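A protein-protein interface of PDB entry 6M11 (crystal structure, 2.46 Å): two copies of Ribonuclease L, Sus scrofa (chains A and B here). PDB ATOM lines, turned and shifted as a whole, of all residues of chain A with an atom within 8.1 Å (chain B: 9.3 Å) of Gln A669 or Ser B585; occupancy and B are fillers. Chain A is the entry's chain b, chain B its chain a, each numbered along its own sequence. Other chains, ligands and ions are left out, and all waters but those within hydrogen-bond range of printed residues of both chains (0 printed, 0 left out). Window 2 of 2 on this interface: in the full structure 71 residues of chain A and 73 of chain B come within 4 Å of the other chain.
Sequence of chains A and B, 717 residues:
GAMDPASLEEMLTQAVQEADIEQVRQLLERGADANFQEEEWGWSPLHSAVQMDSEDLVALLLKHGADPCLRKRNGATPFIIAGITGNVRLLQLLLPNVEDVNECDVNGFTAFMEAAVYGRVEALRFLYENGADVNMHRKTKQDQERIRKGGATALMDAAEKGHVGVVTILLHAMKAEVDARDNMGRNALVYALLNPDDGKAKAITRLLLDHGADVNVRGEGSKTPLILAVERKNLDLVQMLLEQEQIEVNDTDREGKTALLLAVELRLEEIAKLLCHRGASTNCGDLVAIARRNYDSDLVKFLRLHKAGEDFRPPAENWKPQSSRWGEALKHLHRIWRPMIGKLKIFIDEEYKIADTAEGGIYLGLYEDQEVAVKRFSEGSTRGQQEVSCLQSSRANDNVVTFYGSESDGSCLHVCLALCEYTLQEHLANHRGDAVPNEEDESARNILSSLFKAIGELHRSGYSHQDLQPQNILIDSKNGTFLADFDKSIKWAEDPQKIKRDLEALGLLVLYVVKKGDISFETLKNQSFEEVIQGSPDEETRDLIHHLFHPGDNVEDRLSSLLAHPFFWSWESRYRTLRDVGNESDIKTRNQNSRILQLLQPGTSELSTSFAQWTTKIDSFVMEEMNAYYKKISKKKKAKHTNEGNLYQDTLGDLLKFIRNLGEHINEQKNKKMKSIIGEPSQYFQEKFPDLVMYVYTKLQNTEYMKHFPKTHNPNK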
ATOM      1  N   GLU A 625      16.524  -2.795   8.684  1.00  0.00           N
ATOM      2  CA  GLU A 625      16.864  -1.480   9.242  1.00  0.00           C
ATOM      3  C   GLU A 625      18.372  -1.222   9.241  1.00  0.00           C
ATOM      4  O   GLU A 625      18.849  -0.095   8.955  1.00  0.00           O
ATOM      5  CB  GLU A 625      16.319  -1.336  10.640  1.00  0.00           C
ATOM      6  CG  GLU A 625      16.629   0.024  11.223  1.00  0.00           C
ATOM      7  CD  GLU A 625      15.580   0.518  12.200  1.00  0.00           C
ATOM      8  OE1 GLU A 625      14.379   0.196  12.074  1.00  0.00           O
ATOM      9  OE2 GLU A 625      15.951   1.266  13.120  1.00  0.00           O
ATOM     10  N   GLU A 664      27.124   0.713  18.408  1.00  0.00           N
ATOM     11  CA  GLU A 664      27.172   2.157  18.348  1.00  0.00           C
ATOM     12  C   GLU A 664      25.813   2.874  18.321  1.00  0.00           C
ATOM     13  O   GLU A 664      25.662   3.944  18.919  1.00  0.00           O
ATOM     14  CB  GLU A 664      28.058   2.585  17.159  1.00  0.00           C
ATOM     15  CG  GLU A 664      29.562   2.361  17.354  1.00  0.00           C
ATOM     16  CD  GLU A 664      30.068   2.605  18.774  1.00  0.00           C
ATOM     17  OE1 GLU A 664      30.281   3.811  19.133  1.00  0.00           O
ATOM     18  OE2 GLU A 664      30.222   1.565  19.503  1.00  0.00           O
ATOM     19  N   HIS A 665      24.822   2.253  17.687  1.00  0.00           N
ATOM     20  CA  HIS A 665      23.576   2.951  17.353  1.00  0.00           C
ATOM     21  C   HIS A 665      22.347   2.469  18.098  1.00  0.00           C
ATOM     22  O   HIS A 665      21.388   3.207  18.203  1.00  0.00           O
ATOM     23  CB  HIS A 665      23.328   2.893  15.853  1.00  0.00           C
ATOM     24  CG  HIS A 665      24.450   3.462  15.033  1.00  0.00           C
ATOM     25  ND1 HIS A 665      24.945   4.743  15.239  1.00  0.00           N
ATOM     26  CD2 HIS A 665      25.126   2.961  13.975  1.00  0.00           C
ATOM     27  CE1 HIS A 665      25.896   4.992  14.354  1.00  0.00           C
ATOM     28  NE2 HIS A 665      26.030   3.927  13.580  1.00  0.00           N
ATOM     29  N   ILE A 666      22.412   1.272  18.671  1.00  0.00           N
ATOM     30  CA  ILE A 666      21.256   0.614  19.278  1.00  0.00           C
ATOM     31  C   ILE A 666      20.374   1.534  20.145  1.00  0.00           C
ATOM     32  O   ILE A 666      19.173   1.325  20.238  1.00  0.00           O
ATOM     33  CB  ILE A 666      21.689  -0.699  20.036  1.00  0.00           C
ATOM     34  CG1 ILE A 666      20.533  -1.650  20.254  1.00  0.00           C
ATOM     35  CG2 ILE A 666      22.379  -0.412  21.378  1.00  0.00           C
ATOM     36  CD1 ILE A 666      19.951  -2.207  18.968  1.00  0.00           C
ATOM     37  N   ASN A 667      20.986   2.535  20.773  1.00  0.00           N
ATOM     38  CA  ASN A 667      20.291   3.387  21.755  1.00  0.00           C
ATOM     39  C   ASN A 667      19.837   4.744  21.236  1.00  0.00           C
ATOM     40  O   ASN A 667      19.192   5.494  21.985  1.00  0.00           O
ATOM     41  CB  ASN A 667      21.148   3.555  23.013  1.00  0.00           C
ATOM     42  CG  ASN A 667      20.957   2.406  23.980  1.00  0.00           C
ATOM     43  OD1 ASN A 667      19.960   2.374  24.691  1.00  0.00           O
ATOM     44  ND2 ASN A 667      21.907   1.495  24.036  1.00  0.00           N
ATOM     45  N   GLU A 668      20.171   5.066  19.979  1.00  0.00           N
ATOM     46  CA  GLU A 668      19.677   6.258  19.306  1.00  0.00           C
ATOM     47  C   GLU A 668      18.147   6.249  19.228  1.00  0.00           C
ATOM     48  O   GLU A 668      17.534   5.175  19.041  1.00  0.00           O
ATOM     49  CB  GLU A 668      20.296   6.389  17.924  1.00  0.00           C
ATOM     50  CG  GLU A 668      21.710   6.938  17.966  1.00  0.00           C
ATOM     51  CD  GLU A 668      22.377   7.099  16.597  1.00  0.00           C
ATOM     52  OE1 GLU A 668      21.699   7.181  15.544  1.00  0.00           O
ATOM     53  OE2 GLU A 668      23.628   7.175  16.563  1.00  0.00           O
ATOM     54  N   GLN A 669      17.574   7.441  19.435  1.00  0.00           N
ATOM     55  CA  GLN A 669      16.123   7.714  19.442  1.00  0.00           C
ATOM     56  C   GLN A 669      15.315   6.914  18.410  1.00  0.00           C
ATOM     57  O   GLN A 669      14.350   6.242  18.759  1.00  0.00           O
ATOM     58  CB  GLN A 669      15.886   9.234  19.257  1.00  0.00           C
ATOM     59  CG  GLN A 669      14.416   9.662  19.240  1.00  0.00           C
ATOM     60  CD  GLN A 669      13.742   9.643  20.616  1.00  0.00           C
ATOM     61  OE1 GLN A 669      14.404   9.606  21.659  1.00  0.00           O
ATOM     62  NE2 GLN A 669      12.411   9.669  20.619  1.00  0.00           N
ATOM     63  N   LYS A 670      15.764   6.973  17.156  1.00  0.00           N
ATOM     64  CA  LYS A 670      15.086   6.375  16.004  1.00  0.00           C
ATOM     65  C   LYS A 670      15.191   4.842  15.889  1.00  0.00           C
ATOM     66  O   LYS A 670      14.598   4.252  14.993  1.00  0.00           O
ATOM     67  CB  LYS A 670      15.468   7.100  14.681  1.00  0.00           C
ATOM     68  CG  LYS A 670      16.959   7.190  14.288  1.00  0.00           C
ATOM     69  CD  LYS A 670      17.631   8.575  14.415  1.00  0.00           C
ATOM     70  CE  LYS A 670      17.194   9.602  13.378  1.00  0.00           C
ATOM     71  NZ  LYS A 670      18.146   9.565  12.247  1.00  0.00           N
ATOM     72  N   ASN A 671      15.927   4.196  16.787  1.00  0.00           N
ATOM     73  CA  ASN A 671      16.122   2.745  16.716  1.00  0.00           C
ATOM     74  C   ASN A 671      15.452   1.993  17.863  1.00  0.00           C
ATOM     75  O   ASN A 671      15.758   0.823  18.155  1.00  0.00           O
ATOM     76  CB  ASN A 671      17.596   2.383  16.614  1.00  0.00           C
ATOM     77  CG  ASN A 671      18.251   2.862  15.337  1.00  0.00           C
ATOM     78  OD1 ASN A 671      17.683   2.795  14.253  1.00  0.00           O
ATOM     79  ND2 ASN A 671      19.469   3.381  15.477  1.00  0.00           N
ATOM     80  N   LYS A 672      14.453   2.644  18.443  1.00  0.00           N
ATOM     81  CA  LYS A 672      13.740   2.124  19.596  1.00  0.00           C
ATOM     82  C   LYS A 672      13.126   0.726  19.365  1.00  0.00           C
ATOM     83  O   LYS A 672      13.130  -0.089  20.288  1.00  0.00           O
ATOM     84  CB  LYS A 672      12.713   3.161  20.058  1.00  0.00           C
ATOM     85  CG  LYS A 672      12.491   3.204  21.559  1.00  0.00           C
ATOM     86  CD  LYS A 672      11.681   4.444  21.915  1.00  0.00           C
ATOM     87  CE  LYS A 672      11.187   4.411  23.358  1.00  0.00           C
ATOM     88  NZ  LYS A 672      12.247   4.664  24.377  1.00  0.00           N
ATOM     89  N   LYS A 673      12.634   0.462  18.149  1.00  0.00           N
ATOM     90  CA  LYS A 673      11.972  -0.823  17.781  1.00  0.00           C
ATOM     91  C   LYS A 673      12.954  -2.007  17.701  1.00  0.00           C
ATOM     92  O   LYS A 673      12.671  -3.118  18.202  1.00  0.00           O
ATOM     93  CB  LYS A 673      11.169  -0.692  16.463  1.00  0.00           C
ATOM     94  CG  LYS A 673       9.749  -1.251  16.480  1.00  0.00           C
ATOM     95  CD  LYS A 673       9.638  -2.722  16.083  1.00  0.00           C
ATOM     96  CE  LYS A 673       8.244  -3.050  15.565  1.00  0.00           C
ATOM     97  NZ  LYS A 673       7.772  -4.446  15.852  1.00  0.00           N
ATOM     98  N   LYS A 675      15.924  -2.071  19.360  1.00  0.00           N
ATOM     99  CA  LYS A 675      16.303  -2.235  20.761  1.00  0.00           C
ATOM    100  C   LYS A 675      15.429  -3.224  21.542  1.00  0.00           C
ATOM    101  O   LYS A 675      15.956  -4.008  22.323  1.00  0.00           O
ATOM    102  CB  LYS A 675      16.326  -0.862  21.455  1.00  0.00           C
ATOM    103  CG  LYS A 675      17.103  -0.785  22.744  1.00  0.00           C
ATOM    104  CD  LYS A 675      16.495   0.276  23.644  1.00  0.00           C
ATOM    105  CE  LYS A 675      17.409   0.582  24.800  1.00  0.00           C
ATOM    106  NZ  LYS A 675      17.906  -0.655  25.474  1.00  0.00           N
ATOM    107  N   ARG B 579      34.428   8.278  25.852  1.00  0.00           N
ATOM    108  CA  ARG B 579      33.847   7.815  24.583  1.00  0.00           C
ATOM    109  C   ARG B 579      32.438   7.281  24.750  1.00  0.00           C
ATOM    110  O   ARG B 579      31.592   7.544  23.909  1.00  0.00           O
ATOM    111  CB  ARG B 579      34.703   6.712  23.979  1.00  0.00           C
ATOM    112  CG  ARG B 579      35.989   7.243  23.397  1.00  0.00           C
ATOM    113  CD  ARG B 579      36.943   6.149  23.017  1.00  0.00           C
ATOM    114  NE  ARG B 579      36.474   5.405  21.848  1.00  0.00           N
ATOM    115  CZ  ARG B 579      37.056   4.309  21.367  1.00  0.00           C
ATOM    116  NH1 ARG B 579      38.184   3.839  21.906  1.00  0.00           N
ATOM    117  NH2 ARG B 579      36.513   3.696  20.325  1.00  0.00           N
ATOM    118  N   ASP B 580      32.202   6.527  25.826  1.00  0.00           N
ATOM    119  CA  ASP B 580      30.900   5.936  26.101  1.00  0.00           C
ATOM    120  C   ASP B 580      29.860   6.995  26.457  1.00  0.00           C
ATOM    121  O   ASP B 580      28.734   6.948  25.954  1.00  0.00           O
ATOM    122  CB  ASP B 580      31.004   4.891  27.218  1.00  0.00           C
ATOM    123  CG  ASP B 580      31.637   3.570  26.746  1.00  0.00           C
ATOM    124  OD1 ASP B 580      32.068   3.445  25.566  1.00  0.00           O
ATOM    125  OD2 ASP B 580      31.615   2.618  27.580  1.00  0.00           O
ATOM    126  N   VAL B 581      30.251   7.944  27.317  1.00  0.00           N
ATOM    127  CA  VAL B 581      29.404   9.087  27.650  1.00  0.00           C
ATOM    128  C   VAL B 581      29.064   9.832  26.359  1.00  0.00           C
ATOM    129  O   VAL B 581      27.886  10.041  26.067  1.00  0.00           O
ATOM    130  CB  VAL B 581      30.042  10.016  28.703  1.00  0.00           C
ATOM    131  CG1 VAL B 581      29.175  11.240  28.955  1.00  0.00           C
ATOM    132  CG2 VAL B 581      30.191   9.306  30.029  1.00  0.00           C
ATOM    133  N   GLY B 582      30.092  10.179  25.576  1.00  0.00           N
ATOM    134  CA  GLY B 582      29.917  10.838  24.280  1.00  0.00           C
ATOM    135  C   GLY B 582      29.111  10.112  23.206  1.00  0.00           C
ATOM    136  O   GLY B 582      29.007  10.632  22.104  1.00  0.00           O
ATOM    137  N   ASN B 583      28.647   8.894  23.472  1.00  0.00           N
ATOM    138  CA  ASN B 583      27.812   8.143  22.537  1.00  0.00           C
ATOM    139  C   ASN B 583      26.356   8.119  22.952  1.00  0.00           C
ATOM    140  O   ASN B 583      25.536   7.475  22.271  1.00  0.00           O
ATOM    141  CB  ASN B 583      28.316   6.695  22.361  1.00  0.00           C
ATOM    142  CG  ASN B 583      27.795   6.051  21.098  1.00  0.00           C
ATOM    143  OD1 ASN B 583      28.030   6.535  19.993  1.00  0.00           O
ATOM    144  ND2 ASN B 583      27.077   4.954  21.263  1.00  0.00           N
ATOM    145  N   GLU B 584      26.021   8.779  24.063  1.00  0.00           N
ATOM    146  CA  GLU B 584      24.639   8.937  24.502  1.00  0.00           C
ATOM    147  C   GLU B 584      23.874   9.747  23.453  1.00  0.00           C
ATOM    148  O   GLU B 584      24.376  10.761  22.927  1.00  0.00           O
ATOM    149  CB  GLU B 584      24.593   9.619  25.873  1.00  0.00           C
ATOM    150  CG  GLU B 584      24.754   8.662  27.062  1.00  0.00           C
ATOM    151  CD  GLU B 584      23.478   7.888  27.408  1.00  0.00           C
ATOM    152  OE1 GLU B 584      22.385   8.192  26.865  1.00  0.00           O
ATOM    153  OE2 GLU B 584      23.535   6.975  28.263  1.00  0.00           O
ATOM    154  N   SER B 585      22.677   9.262  23.142  1.00  0.00           N
ATOM    155  CA  SER B 585      21.795   9.859  22.137  1.00  0.00           C
ATOM    156  C   SER B 585      21.660  11.386  22.270  1.00  0.00           C
ATOM    157  O   SER B 585      21.788  12.124  21.294  1.00  0.00           O
ATOM    158  CB  SER B 585      20.398   9.242  22.228  1.00  0.00           C
ATOM    159  OG  SER B 585      20.413   7.859  21.968  1.00  0.00           O
ATOM    160  N   ASP B 586      21.458  11.840  23.502  1.00  0.00           N
ATOM    161  CA  ASP B 586      21.137  13.238  23.778  1.00  0.00           C
ATOM    162  C   ASP B 586      22.345  14.158  23.715  1.00  0.00           C
ATOM    163  O   ASP B 586      22.187  15.373  23.582  1.00  0.00           O
ATOM    164  CB  ASP B 586      20.465  13.341  25.143  1.00  0.00           C
ATOM    165  CG  ASP B 586      19.453  12.218  25.412  1.00  0.00           C
ATOM    166  OD1 ASP B 586      19.627  11.022  25.027  1.00  0.00           O
ATOM    167  OD2 ASP B 586      18.446  12.529  26.083  1.00  0.00           O
ATOM    168  N   ILE B 587      23.552  13.589  23.817  1.00  0.00           N
ATOM    169  CA  ILE B 587      24.774  14.334  23.501  1.00  0.00           C
ATOM    170  C   ILE B 587      24.910  14.487  21.984  1.00  0.00           C
ATOM    171  O   ILE B 587      25.204  15.579  21.500  1.00  0.00           O
ATOM    172  CB  ILE B 587      26.014  13.725  24.194  1.00  0.00           C
ATOM    173  CG1 ILE B 587      26.003  14.147  25.670  1.00  0.00           C
ATOM    174  CG2 ILE B 587      27.318  14.195  23.543  1.00  0.00           C
ATOM    175  CD1 ILE B 587      26.965  13.409  26.552  1.00  0.00           C
ATOM    176  N   LYS B 588      24.658  13.410  21.244  1.00  0.00           N
ATOM    177  CA  LYS B 588      24.737  13.440  19.764  1.00  0.00           C
ATOM    178  C   LYS B 588      23.660  14.305  19.082  1.00  0.00           C
ATOM    179  O   LYS B 588      23.960  15.015  18.118  1.00  0.00           O
ATOM    180  CB  LYS B 588      24.796  12.026  19.158  1.00  0.00           C
ATOM    181  CG  LYS B 588      26.090  11.265  19.450  1.00  0.00           C
ATOM    182  CD  LYS B 588      26.141   9.912  18.747  1.00  0.00           C
ATOM    183  CE  LYS B 588      25.091   8.953  19.287  1.00  0.00           C
ATOM    184  NZ  LYS B 588      25.407   7.528  19.002  1.00  0.00           N
ATOM    185  N   THR B 589      22.426  14.261  19.592  1.00  0.00           N
ATOM    186  CA  THR B 589      21.333  15.115  19.068  1.00  0.00           C
ATOM    187  C   THR B 589      21.336  16.530  19.688  1.00  0.00           C
ATOM    188  O   THR B 589      20.490  17.354  19.342  1.00  0.00           O
ATOM    189  CB  THR B 589      19.920  14.471  19.234  1.00  0.00           C
ATOM    190  OG1 THR B 589      19.547  14.420  20.621  1.00  0.00           O
ATOM    191  CG2 THR B 589      19.851  13.059  18.625  1.00  0.00           C
ATOM    192  N   ARG B 590      22.290  16.791  20.590  1.00  0.00           N
ATOM    193  CA  ARG B 590      22.393  18.039  21.371  1.00  0.00           C
ATOM    194  C   ARG B 590      21.077  18.466  22.064  1.00  0.00           C
ATOM    195  O   ARG B 590      20.731  19.669  22.102  1.00  0.00           O
ATOM    196  CB  ARG B 590      23.000  19.156  20.534  1.00  0.00           C
ATOM    197  CG  ARG B 590      23.808  20.156  21.358  1.00  0.00           C
ATOM    198  CD  ARG B 590      24.297  21.359  20.552  1.00  0.00           C
ATOM    199  NE  ARG B 590      25.399  21.053  19.621  1.00  0.00           N
ATOM    200  CZ  ARG B 590      25.314  21.111  18.288  1.00  0.00           C
ATOM    201  NH1 ARG B 590      24.179  21.462  17.690  1.00  0.00           N
ATOM    202  NH2 ARG B 590      26.362  20.822  17.535  1.00  0.00           N
ATOM    203  N   ASN B 591      20.361  17.489  22.631  1.00  0.00           N
ATOM    204  CA  ASN B 591      19.119  17.738  23.347  1.00  0.00           C
ATOM    205  C   ASN B 591      19.361  18.479  24.672  1.00  0.00           C
ATOM    206  O   ASN B 591      19.698  17.866  25.694  1.00  0.00           O
ATOM    207  CB  ASN B 591      18.356  16.425  23.603  1.00  0.00           C
ATOM    208  CG  ASN B 591      17.011  16.653  24.286  1.00  0.00           C
ATOM    209  OD1 ASN B 591      16.336  17.635  23.989  1.00  0.00           O
ATOM    210  ND2 ASN B 591      16.647  15.790  25.251  1.00  0.00           N
ATOM    211  N   GLN B 592      19.116  19.795  24.649  1.00  0.00           N
ATOM    212  CA  GLN B 592      19.194  20.681  25.813  1.00  0.00           C
ATOM    213  C   GLN B 592      18.270  20.304  26.988  1.00  0.00           C
ATOM    214  O   GLN B 592      18.586  20.626  28.141  1.00  0.00           O
ATOM    215  CB  GLN B 592      18.895  22.121  25.365  1.00  0.00           C
ATOM    216  CG  GLN B 592      19.324  23.217  26.337  1.00  0.00           C
ATOM    217  CD  GLN B 592      20.801  23.563  26.270  1.00  0.00           C
ATOM    218  OE1 GLN B 592      21.655  22.716  26.014  1.00  0.00           O
ATOM    219  NE2 GLN B 592      21.106  24.827  26.524  1.00  0.00           N
ATOM    220  N   SER B 594      17.548  17.113  27.907  1.00  0.00           N
ATOM    221  CA  SER B 594      17.894  15.796  28.447  1.00  0.00           C
ATOM    222  C   SER B 594      18.527  15.786  29.815  1.00  0.00           C
ATOM    223  O   SER B 594      19.207  16.723  30.227  1.00  0.00           O
ATOM    224  CB  SER B 594      18.860  15.104  27.517  1.00  0.00           C
ATOM    225  OG  SER B 594      20.066  15.826  27.401  1.00  0.00           O
ATOM    226  N   ILE B 596      21.037  13.937  30.893  1.00  0.00           N
ATOM    227  CA  ILE B 596      22.516  13.927  30.791  1.00  0.00           C
ATOM    228  C   ILE B 596      23.111  15.347  30.711  1.00  0.00           C
ATOM    229  O   ILE B 596      24.018  15.698  31.489  1.00  0.00           O
ATOM    230  CB  ILE B 596      23.017  13.011  29.631  1.00  0.00           C
ATOM    231  CG1 ILE B 596      24.555  12.955  29.548  1.00  0.00           C
ATOM    232  CG2 ILE B 596      22.467  13.455  28.271  1.00  0.00           C
ATOM    233  CD1 ILE B 596      25.205  11.970  30.483  1.00  0.00           C
ATOM    234  N   LEU B 597      22.615  16.164  29.779  1.00  0.00           N
ATOM    235  CA  LEU B 597      23.135  17.508  29.585  1.00  0.00           C
ATOM    236  C   LEU B 597      22.731  18.465  30.703  1.00  0.00           C
ATOM    237  O   LEU B 597      23.431  19.451  30.957  1.00  0.00           O
ATOM    238  CB  LEU B 597      22.767  18.058  28.200  1.00  0.00           C
ATOM    239  CG  LEU B 597      23.629  17.520  27.043  1.00  0.00           C
ATOM    240  CD1 LEU B 597      23.059  17.876  25.696  1.00  0.00           C
ATOM    241  CD2 LEU B 597      25.057  18.029  27.160  1.00  0.00           C
ATOM    242  N   GLY B 653      29.340  18.771  26.385  1.00  0.00           N
ATOM    243  CA  GLY B 653      28.644  17.794  25.566  1.00  0.00           C
ATOM    244  C   GLY B 653      29.319  17.602  24.210  1.00  0.00           C
ATOM    245  O   GLY B 653      29.562  16.460  23.770  1.00  0.00           O
ATOM    246  N   ASP B 654      29.655  18.711  23.557  1.00  0.00           N
ATOM    247  CA  ASP B 654      30.330  18.629  22.253  1.00  0.00           C
ATOM    248  C   ASP B 654      31.800  18.182  22.323  1.00  0.00           C
ATOM    249  O   ASP B 654      32.323  17.665  21.356  1.00  0.00           O
ATOM    250  CB  ASP B 654      30.134  19.907  21.427  1.00  0.00           C
ATOM    251  CG  ASP B 654      28.696  20.041  20.866  1.00  0.00           C
ATOM    252  OD1 ASP B 654      27.878  19.067  20.867  1.00  0.00           O
ATOM    253  OD2 ASP B 654      28.377  21.145  20.387  1.00  0.00           O
ATOM    254  N   LYS B 657      31.301  14.282  22.680  1.00  0.00           N
ATOM    255  CA  LYS B 657      30.962  13.836  21.299  1.00  0.00           C
ATOM    256  C   LYS B 657      32.214  13.849  20.394  1.00  0.00           C
ATOM    257  O   LYS B 657      32.405  12.926  19.594  1.00  0.00           O
ATOM    258  CB  LYS B 657      29.815  14.703  20.713  1.00  0.00           C
ATOM    259  CG  LYS B 657      29.596  14.633  19.205  1.00  0.00           C
ATOM    260  CD  LYS B 657      28.115  14.688  18.857  1.00  0.00           C
ATOM    261  CE  LYS B 657      27.497  16.082  18.813  1.00  0.00           C
ATOM    262  NZ  LYS B 657      28.227  17.084  17.983  1.00  0.00           N
ATOM    263  N   ARG B 660      34.142  10.870  21.301  1.00  0.00           N
ATOM    264  CA  ARG B 660      33.481   9.696  20.760  1.00  0.00           C
ATOM    265  C   ARG B 660      33.814   9.463  19.285  1.00  0.00           C
ATOM    266  O   ARG B 660      34.203   8.357  18.897  1.00  0.00           O
ATOM    267  CB  ARG B 660      31.982   9.805  20.941  1.00  0.00           C
ATOM    268  CG  ARG B 660      31.288   8.478  20.703  1.00  0.00           C
ATOM    269  CD  ARG B 660      30.125   8.564  19.733  1.00  0.00           C
ATOM    270  NE  ARG B 660      30.568   8.642  18.343  1.00  0.00           N
ATOM    271  CZ  ARG B 660      30.280   7.788  17.368  1.00  0.00           C
ATOM    272  NH1 ARG B 660      29.492   6.719  17.556  1.00  0.00           N
ATOM    273  NH2 ARG B 660      30.802   8.045  16.182  1.00  0.00           N
ATOM    274  N   TYR B 705      23.965   7.280  34.697  1.00  0.00           N
ATOM    275  CA  TYR B 705      25.071   7.192  33.729  1.00  0.00           C
ATOM    276  C   TYR B 705      26.431   6.907  34.406  1.00  0.00           C
ATOM    277  O   TYR B 705      27.471   6.850  33.742  1.00  0.00           O
ATOM    278  CB  TYR B 705      25.188   8.459  32.882  1.00  0.00           C
ATOM    279  CG  TYR B 705      23.887   9.044  32.418  1.00  0.00           C
ATOM    280  CD1 TYR B 705      23.258   8.545  31.279  1.00  0.00           C
ATOM    281  CD2 TYR B 705      23.283  10.098  33.111  1.00  0.00           C
ATOM    282  CE1 TYR B 705      22.042   9.074  30.844  1.00  0.00           C
ATOM    283  CE2 TYR B 705      22.079  10.622  32.678  1.00  0.00           C
ATOM    284  CZ  TYR B 705      21.463  10.112  31.543  1.00  0.00           C
ATOM    285  OH  TYR B 705      20.271  10.656  31.111  1.00  0.00           O
ATOM    286  N   HIS B 708      28.528   3.979  32.848  1.00  0.00           N
ATOM    287  CA  HIS B 708      29.587   4.158  31.888  1.00  0.00           C
ATOM    288  C   HIS B 708      30.984   4.124  32.476  1.00  0.00           C
ATOM    289  O   HIS B 708      31.959   4.102  31.734  1.00  0.00           O
ATOM    290  CB  HIS B 708      29.392   5.468  31.188  1.00  0.00           C
ATOM    291  CG  HIS B 708      28.198   5.491  30.302  1.00  0.00           C
ATOM    292  ND1 HIS B 708      27.850   4.425  29.498  1.00  0.00           N
ATOM    293  CD2 HIS B 708      27.272   6.455  30.083  1.00  0.00           C
ATOM    294  CE1 HIS B 708      26.758   4.737  28.822  1.00  0.00           C
ATOM    295  NE2 HIS B 708      26.393   5.966  29.154  1.00  0.00           N
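Of the 23 printed residues of chain B, 4 touch a printed residue of chain A.
Printed residues of chain B that touch a printed residue of chain A: Asn B583, Ser B585, Lys B588 and Arg B660.
Along chain A the printed residues that touch a printed residue of chain B span positions 664 to 669.
Among the printed residues, 7 pairs touch across the chains.
Among the printed residues, Asp or Glu carboxylates within 4 Å of a Lys or Arg side-chain nitrogen of the other chain: Glu A664 with Arg B660 (3.4 Å) and Glu A668 with Lys B588 (3.0 Å).
No position is printed for both chains.
Ser B585 touches just these residues of chain A: Asn A667 (2.7 Å), Glu A668 (3.2 Å) and Gln A669 (3.8 Å).
Printed residues of chain A within 4 Å of Arg B660: Glu A664.
Of the printed residues of chain B, Glu A668 touches Ser B585 and Lys B588.
Of the printed residues of chain A, Asn B583 touches Glu A664.
The nearest residue of chain B that does not touch Gln A669 is Thr B589 (5.5 Å).
Among the printed residues, pairs that only touch across the chains: Glu A664 with Lys B588 and Gln A669 with Ser B585.
The side-chain amide oxygen (OD1) of Asn B583 sits at hydrogen-bond distance from the side-chain amino group (NZ) of Lys B588 (3.0 Å).
ND1 of His A665 lies within hydrogen-bond range of OE2 of Glu A668, 3.1 Å away.
The guanidinium group (NH1) of Arg B660 lies within hydrogen-bond range of the side-chain amide oxygen (OD1) of Asn B583 (2.8 Å).
O of Ser B585 lies within hydrogen-bond range of OG1 of Thr B589, 3.3 Å away.
ND2 of Asn B583 sits at hydrogen-bond distance from O of Glu A664 (2.9 Å).
The side-chain carboxylate (OE1) of Glu A664 is in salt-bridge range of the guanidinium group (NH1) of Arg B660.
N of Glu A668 sits close to OG of Ser B585, at 3.4 Å.
NZ of Lys B588 lies within salt-bridge range of OE2 of Glu A668, at 3.0 Å.
O of Asn A667 sits at hydrogen-bond distance from OG of Ser B585.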
